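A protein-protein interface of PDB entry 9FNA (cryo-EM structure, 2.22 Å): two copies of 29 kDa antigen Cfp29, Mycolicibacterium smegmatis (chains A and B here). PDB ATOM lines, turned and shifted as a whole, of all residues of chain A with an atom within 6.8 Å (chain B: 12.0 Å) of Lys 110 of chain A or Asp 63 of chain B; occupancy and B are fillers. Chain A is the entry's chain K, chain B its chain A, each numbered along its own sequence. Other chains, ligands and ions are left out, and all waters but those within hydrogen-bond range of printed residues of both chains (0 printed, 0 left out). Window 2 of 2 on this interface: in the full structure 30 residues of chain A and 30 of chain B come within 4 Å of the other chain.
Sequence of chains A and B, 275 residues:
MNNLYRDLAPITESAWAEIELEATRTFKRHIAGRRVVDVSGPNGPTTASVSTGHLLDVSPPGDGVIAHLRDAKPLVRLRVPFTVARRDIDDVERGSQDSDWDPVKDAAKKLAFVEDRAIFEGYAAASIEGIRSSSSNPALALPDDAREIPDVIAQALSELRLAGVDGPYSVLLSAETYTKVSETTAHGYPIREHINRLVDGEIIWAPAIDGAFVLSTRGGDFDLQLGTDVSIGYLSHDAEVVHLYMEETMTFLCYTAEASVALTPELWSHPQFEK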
ATOM      1  N   PHE A  27     -24.523   0.727  -9.467  1.00  0.00           N
ATOM      2  CA  PHE A  27     -24.710  -0.210  -8.365  1.00  0.00           C
ATOM      3  C   PHE A  27     -24.827   0.525  -7.037  1.00  0.00           C
ATOM      4  O   PHE A  27     -25.707   0.219  -6.222  1.00  0.00           O
ATOM      5  CB  PHE A  27     -23.555  -1.210  -8.330  1.00  0.00           C
ATOM      6  CG  PHE A  27     -23.774  -2.356  -7.385  1.00  0.00           C
ATOM      7  CD1 PHE A  27     -23.320  -2.293  -6.080  1.00  0.00           C
ATOM      8  CD2 PHE A  27     -24.433  -3.497  -7.804  1.00  0.00           C
ATOM      9  CE1 PHE A  27     -23.521  -3.346  -5.212  1.00  0.00           C
ATOM     10  CE2 PHE A  27     -24.638  -4.553  -6.940  1.00  0.00           C
ATOM     11  CZ  PHE A  27     -24.180  -4.477  -5.642  1.00  0.00           C
ATOM     12  N   VAL A  80     -23.959 -12.107 -13.723  1.00  0.00           N
ATOM     13  CA  VAL A  80     -24.901 -11.513 -14.670  1.00  0.00           C
ATOM     14  C   VAL A  80     -24.148 -11.180 -15.954  1.00  0.00           C
ATOM     15  O   VAL A  80     -23.244 -10.332 -15.929  1.00  0.00           O
ATOM     16  CB  VAL A  80     -25.574 -10.262 -14.084  1.00  0.00           C
ATOM     17  CG1 VAL A  80     -26.592  -9.702 -15.065  1.00  0.00           C
ATOM     18  CG2 VAL A  80     -26.236 -10.586 -12.755  1.00  0.00           C
ATOM     19  N   PRO A  81     -24.458 -11.820 -17.078  1.00  0.00           N
ATOM     20  CA  PRO A  81     -23.745 -11.522 -18.322  1.00  0.00           C
ATOM     21  C   PRO A  81     -24.376 -10.374 -19.098  1.00  0.00           C
ATOM     22  O   PRO A  81     -25.571 -10.091 -18.995  1.00  0.00           O
ATOM     23  CB  PRO A  81     -23.852 -12.832 -19.105  1.00  0.00           C
ATOM     24  CG  PRO A  81     -25.146 -13.409 -18.665  1.00  0.00           C
ATOM     25  CD  PRO A  81     -25.351 -12.983 -17.232  1.00  0.00           C
ATOM     26  N   LYS A 105     -25.159  -0.707 -17.307  1.00  0.00           N
ATOM     27  CA  LYS A 105     -26.036  -0.185 -16.265  1.00  0.00           C
ATOM     28  C   LYS A 105     -27.131  -1.188 -15.918  1.00  0.00           C
ATOM     29  O   LYS A 105     -27.463  -1.377 -14.741  1.00  0.00           O
ATOM     30  CB  LYS A 105     -26.637   1.147 -16.711  1.00  0.00           C
ATOM     31  CG  LYS A 105     -25.679   2.319 -16.567  1.00  0.00           C
ATOM     32  CD  LYS A 105     -25.671   3.207 -17.804  1.00  0.00           C
ATOM     33  CE  LYS A 105     -27.015   3.883 -18.038  1.00  0.00           C
ATOM     34  NZ  LYS A 105     -27.616   4.413 -16.784  1.00  0.00           N
ATOM     35  N   ASP A 106     -27.702  -1.842 -16.931  1.00  0.00           N
ATOM     36  CA  ASP A 106     -28.756  -2.820 -16.685  1.00  0.00           C
ATOM     37  C   ASP A 106     -28.237  -4.003 -15.878  1.00  0.00           C
ATOM     38  O   ASP A 106     -28.910  -4.477 -14.954  1.00  0.00           O
ATOM     39  CB  ASP A 106     -29.345  -3.300 -18.010  1.00  0.00           C
ATOM     40  CG  ASP A 106     -30.145  -2.225 -18.717  1.00  0.00           C
ATOM     41  OD1 ASP A 106     -30.170  -1.079 -18.222  1.00  0.00           O
ATOM     42  OD2 ASP A 106     -30.747  -2.527 -19.768  1.00  0.00           O
ATOM     43  N   ALA A 107     -27.048  -4.504 -16.219  1.00  0.00           N
ATOM     44  CA  ALA A 107     -26.482  -5.620 -15.468  1.00  0.00           C
ATOM     45  C   ALA A 107     -26.204  -5.223 -14.025  1.00  0.00           C
ATOM     46  O   ALA A 107     -26.455  -6.002 -13.096  1.00  0.00           O
ATOM     47  CB  ALA A 107     -25.206  -6.113 -16.146  1.00  0.00           C
ATOM     48  N   ALA A 108     -25.674  -4.014 -13.815  1.00  0.00           N
ATOM     49  CA  ALA A 108     -25.441  -3.549 -12.452  1.00  0.00           C
ATOM     50  C   ALA A 108     -26.749  -3.464 -11.674  1.00  0.00           C
ATOM     51  O   ALA A 108     -26.815  -3.870 -10.505  1.00  0.00           O
ATOM     52  CB  ALA A 108     -24.741  -2.191 -12.477  1.00  0.00           C
ATOM     53  N   LYS A 109     -27.800  -2.939 -12.308  1.00  0.00           N
ATOM     54  CA  LYS A 109     -29.102  -2.870 -11.655  1.00  0.00           C
ATOM     55  C   LYS A 109     -29.597  -4.260 -11.283  1.00  0.00           C
ATOM     56  O   LYS A 109     -30.111  -4.473 -10.178  1.00  0.00           O
ATOM     57  CB  LYS A 109     -30.110  -2.185 -12.576  1.00  0.00           C
ATOM     58  CG  LYS A 109     -30.362  -0.720 -12.267  1.00  0.00           C
ATOM     59  CD  LYS A 109     -31.178  -0.045 -13.367  1.00  0.00           C
ATOM     60  CE  LYS A 109     -32.452  -0.810 -13.699  1.00  0.00           C
ATOM     61  NZ  LYS A 109     -33.210  -1.202 -12.479  1.00  0.00           N
ATOM     62  N   LYS A 110     -29.454  -5.217 -12.201  1.00  0.00           N
ATOM     63  CA  LYS A 110     -29.914  -6.577 -11.947  1.00  0.00           C
ATOM     64  C   LYS A 110     -29.177  -7.191 -10.764  1.00  0.00           C
ATOM     65  O   LYS A 110     -29.793  -7.817  -9.888  1.00  0.00           O
ATOM     66  CB  LYS A 110     -29.706  -7.418 -13.207  1.00  0.00           C
ATOM     67  CG  LYS A 110     -30.504  -8.722 -13.255  1.00  0.00           C
ATOM     68  CD  LYS A 110     -31.206  -9.002 -14.605  1.00  0.00           C
ATOM     69  CE  LYS A 110     -30.507  -8.388 -15.823  1.00  0.00           C
ATOM     70  NZ  LYS A 110     -31.113  -8.822 -17.114  1.00  0.00           N
ATOM     71  N   LEU A 111     -27.853  -7.023 -10.723  1.00  0.00           N
ATOM     72  CA  LEU A 111     -27.069  -7.581  -9.625  1.00  0.00           C
ATOM     73  C   LEU A 111     -27.454  -6.943  -8.296  1.00  0.00           C
ATOM     74  O   LEU A 111     -27.620  -7.639  -7.283  1.00  0.00           O
ATOM     75  CB  LEU A 111     -25.578  -7.393  -9.902  1.00  0.00           C
ATOM     76  CG  LEU A 111     -24.612  -8.189  -9.022  1.00  0.00           C
ATOM     77  CD1 LEU A 111     -24.665  -9.670  -9.354  1.00  0.00           C
ATOM     78  CD2 LEU A 111     -23.197  -7.663  -9.181  1.00  0.00           C
ATOM     79  N   ALA A 112     -27.608  -5.617  -8.277  1.00  0.00           N
ATOM     80  CA  ALA A 112     -28.019  -4.947  -7.050  1.00  0.00           C
ATOM     81  C   ALA A 112     -29.381  -5.445  -6.592  1.00  0.00           C
ATOM     82  O   ALA A 112     -29.604  -5.660  -5.394  1.00  0.00           O
ATOM     83  CB  ALA A 112     -28.049  -3.434  -7.259  1.00  0.00           C
ATOM     84  N   PHE A 113     -30.307  -5.632  -7.533  1.00  0.00           N
ATOM     85  CA  PHE A 113     -31.649  -6.067  -7.169  1.00  0.00           C
ATOM     86  C   PHE A 113     -31.627  -7.469  -6.581  1.00  0.00           C
ATOM     87  O   PHE A 113     -32.291  -7.739  -5.575  1.00  0.00           O
ATOM     88  CB  PHE A 113     -32.571  -6.003  -8.385  1.00  0.00           C
ATOM     89  CG  PHE A 113     -33.203  -4.656  -8.593  1.00  0.00           C
ATOM     90  CD1 PHE A 113     -32.546  -3.499  -8.209  1.00  0.00           C
ATOM     91  CD2 PHE A 113     -34.458  -4.547  -9.164  1.00  0.00           C
ATOM     92  CE1 PHE A 113     -33.124  -2.262  -8.397  1.00  0.00           C
ATOM     93  CE2 PHE A 113     -35.042  -3.311  -9.353  1.00  0.00           C
ATOM     94  CZ  PHE A 113     -34.374  -2.167  -8.969  1.00  0.00           C
ATOM     95  N   VAL A 114     -30.869  -8.383  -7.192  1.00  0.00           N
ATOM     96  CA  VAL A 114     -30.812  -9.738  -6.649  1.00  0.00           C
ATOM     97  C   VAL A 114     -30.179  -9.729  -5.262  1.00  0.00           C
ATOM     98  O   VAL A 114     -30.648 -10.420  -4.349  1.00  0.00           O
ATOM     99  CB  VAL A 114     -30.076 -10.695  -7.606  1.00  0.00           C
ATOM    100  CG1 VAL A 114     -30.842 -10.832  -8.907  1.00  0.00           C
ATOM    101  CG2 VAL A 114     -28.664 -10.231  -7.871  1.00  0.00           C
ATOM    102  N   GLU A 115     -29.117  -8.941  -5.072  1.00  0.00           N
ATOM    103  CA  GLU A 115     -28.478  -8.885  -3.760  1.00  0.00           C
ATOM    104  C   GLU A 115     -29.445  -8.361  -2.702  1.00  0.00           C
ATOM    105  O   GLU A 115     -29.595  -8.954  -1.625  1.00  0.00           O
ATOM    106  CB  GLU A 115     -27.226  -8.008  -3.826  1.00  0.00           C
ATOM    107  CG  GLU A 115     -26.315  -8.136  -2.613  1.00  0.00           C
ATOM    108  CD  GLU A 115     -25.518  -6.876  -2.339  1.00  0.00           C
ATOM    109  OE1 GLU A 115     -24.513  -6.642  -3.041  1.00  0.00           O
ATOM    110  OE2 GLU A 115     -25.895  -6.122  -1.417  1.00  0.00           O
ATOM    111  N   VAL B  58     -27.267 -24.346  -9.058  1.00  0.00           N
ATOM    112  CA  VAL B  58     -28.377 -23.993  -8.185  1.00  0.00           C
ATOM    113  C   VAL B  58     -29.353 -23.111  -8.954  1.00  0.00           C
ATOM    114  O   VAL B  58     -28.978 -22.387  -9.879  1.00  0.00           O
ATOM    115  CB  VAL B  58     -27.886 -23.282  -6.902  1.00  0.00           C
ATOM    116  CG1 VAL B  58     -27.276 -21.928  -7.232  1.00  0.00           C
ATOM    117  CG2 VAL B  58     -29.013 -23.139  -5.899  1.00  0.00           C
ATOM    118  N   SER B  59     -30.620 -23.185  -8.560  1.00  0.00           N
ATOM    119  CA  SER B  59     -31.659 -22.421  -9.236  1.00  0.00           C
ATOM    120  C   SER B  59     -31.387 -20.925  -9.093  1.00  0.00           C
ATOM    121  O   SER B  59     -31.049 -20.464  -7.995  1.00  0.00           O
ATOM    122  CB  SER B  59     -33.031 -22.762  -8.661  1.00  0.00           C
ATOM    123  OG  SER B  59     -34.062 -22.423  -9.571  1.00  0.00           O
ATOM    124  N   PRO B  60     -31.525 -20.137 -10.164  1.00  0.00           N
ATOM    125  CA  PRO B  60     -31.182 -18.720 -10.070  1.00  0.00           C
ATOM    126  C   PRO B  60     -32.237 -17.952  -9.294  1.00  0.00           C
ATOM    127  O   PRO B  60     -33.407 -18.365  -9.235  1.00  0.00           O
ATOM    128  CB  PRO B  60     -31.134 -18.272 -11.541  1.00  0.00           C
ATOM    129  CG  PRO B  60     -32.064 -19.195 -12.234  1.00  0.00           C
ATOM    130  CD  PRO B  60     -31.957 -20.512 -11.521  1.00  0.00           C
ATOM    131  N   PRO B  61     -31.868 -16.825  -8.679  1.00  0.00           N
ATOM    132  CA  PRO B  61     -32.898 -15.952  -8.093  1.00  0.00           C
ATOM    133  C   PRO B  61     -33.885 -15.423  -9.115  1.00  0.00           C
ATOM    134  O   PRO B  61     -35.069 -15.257  -8.795  1.00  0.00           O
ATOM    135  CB  PRO B  61     -32.081 -14.815  -7.465  1.00  0.00           C
ATOM    136  CG  PRO B  61     -30.716 -15.363  -7.291  1.00  0.00           C
ATOM    137  CD  PRO B  61     -30.509 -16.327  -8.413  1.00  0.00           C
ATOM    138  N   GLY B  62     -33.437 -15.153 -10.334  1.00  0.00           N
ATOM    139  CA  GLY B  62     -34.307 -14.550 -11.321  1.00  0.00           C
ATOM    140  C   GLY B  62     -33.720 -14.651 -12.710  1.00  0.00           C
ATOM    141  O   GLY B  62     -32.738 -15.356 -12.943  1.00  0.00           O
ATOM    142  N   ASP B  63     -34.347 -13.928 -13.634  1.00  0.00           N
ATOM    143  CA  ASP B  63     -33.960 -13.998 -15.036  1.00  0.00           C
ATOM    144  C   ASP B  63     -32.622 -13.307 -15.268  1.00  0.00           C
ATOM    145  O   ASP B  63     -32.299 -12.305 -14.624  1.00  0.00           O
ATOM    146  CB  ASP B  63     -35.037 -13.355 -15.909  1.00  0.00           C
ATOM    147  CG  ASP B  63     -36.292 -14.198 -16.001  1.00  0.00           C
ATOM    148  OD1 ASP B  63     -37.399 -13.621 -15.988  1.00  0.00           O
ATOM    149  OD2 ASP B  63     -36.172 -15.438 -16.083  1.00  0.00           O
ATOM    150  N   GLY B  64     -31.843 -13.852 -16.199  1.00  0.00           N
ATOM    151  CA  GLY B  64     -30.570 -13.260 -16.556  1.00  0.00           C
ATOM    152  C   GLY B  64     -29.488 -13.409 -15.516  1.00  0.00           C
ATOM    153  O   GLY B  64     -28.485 -12.694 -15.577  1.00  0.00           O
ATOM    154  N   VAL B  65     -29.658 -14.319 -14.560  1.00  0.00           N
ATOM    155  CA  VAL B  65     -28.713 -14.506 -13.468  1.00  0.00           C
ATOM    156  C   VAL B  65     -28.287 -15.965 -13.433  1.00  0.00           C
ATOM    157  O   VAL B  65     -29.126 -16.870 -13.510  1.00  0.00           O
ATOM    158  CB  VAL B  65     -29.321 -14.085 -12.113  1.00  0.00           C
ATOM    159  CG1 VAL B  65     -28.276 -14.162 -11.016  1.00  0.00           C
ATOM    160  CG2 VAL B  65     -29.896 -12.682 -12.203  1.00  0.00           C
ATOM    161  N   ILE B  66     -26.982 -16.191 -13.319  1.00  0.00           N
ATOM    162  CA  ILE B  66     -26.408 -17.527 -13.201  1.00  0.00           C
ATOM    163  C   ILE B  66     -25.888 -17.675 -11.778  1.00  0.00           C
ATOM    164  O   ILE B  66     -25.097 -16.846 -11.310  1.00  0.00           O
ATOM    165  CB  ILE B  66     -25.292 -17.759 -14.230  1.00  0.00           C
ATOM    166  CG1 ILE B  66     -25.837 -17.601 -15.651  1.00  0.00           C
ATOM    167  CG2 ILE B  66     -24.688 -19.142 -14.054  1.00  0.00           C
ATOM    168  CD1 ILE B  66     -24.765 -17.415 -16.698  1.00  0.00           C
ATOM    169  N   ALA B  67     -26.325 -18.729 -11.094  1.00  0.00           N
ATOM    170  CA  ALA B  67     -26.027 -18.932  -9.683  1.00  0.00           C
ATOM    171  C   ALA B  67     -25.280 -20.243  -9.488  1.00  0.00           C
ATOM    172  O   ALA B  67     -25.620 -21.257 -10.108  1.00  0.00           O
ATOM    173  CB  ALA B  67     -27.312 -18.934  -8.854  1.00  0.00           C
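Among the printed residues, pairs that only touch across the chains: Lys 110 of chain A with Asp 63 of chain B (3.5 Å), Pro 81 of chain A with Gly 64 of chain B (3.6 Å), Val 80 of chain A with Gly 64 of chain B (3.6 Å) and Val 114 of chain A with Val 65 of chain B (3.9 Å).
Of chain B, only Asp 63 (3.5 Å) comes within 4 Å of Lys 110 of chain A. Asp 63 of chain B touches one residue of chain A. Val 80 of chain A touches just one residue of chain B: Gly 64. No residue of chain B comes within 4 Å of Asp 106 of chain A. No residue of chain B comes within 4 Å of Ala 107 of chain A. No residue of chain B comes within 4 Å of Ala 108 of chain A. No residue of chain B comes within 4 Å of Lys 109 of chain A. Ala 112 of chain A touches none of the printed residues of chain B. No residue of chain B comes within 4 Å of Phe 113 of chain A. Of the printed residues of chain B, Val 114 of chain A touches Val 65. Printed residues of chain A within 4 Å of Gly 64 of chain B: Val 80 and Pro 81. Printed residues of chain A within 4 Å of Val 65 of chain B: Val 114. Phe 27 of chain A touches none of the printed residues of chain B. Ala 67 of chain B touches none of the printed residues of chain A. The nearest residue of chain B that does not touch Lys 110 of chain A is Val 65 of chain B (4.1 Å). The nearest residue of chain A that does not touch Asp 63 of chain B is Val 114 of chain A (6.1 Å). The nearest printed residue of chain B that does not touch Pro 81 of chain A is Ile 66 of chain B (4.5 Å).
Of the 10 printed residues of chain B, 3 touch a printed residue of chain A. Of the 14 printed residues of chain A, 4 touch a printed residue of chain B. Among the printed residues, 4 pairs touch across the chains. Among the printed residues, no Asp or Glu carboxylate lies within 4 Å of a Lys or Arg side-chain nitrogen of the other chain.
No position is printed for both chains. Of the 4 pairs that touch across the chains among the printed residues, none has its exchanged pair printed and touching as well.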
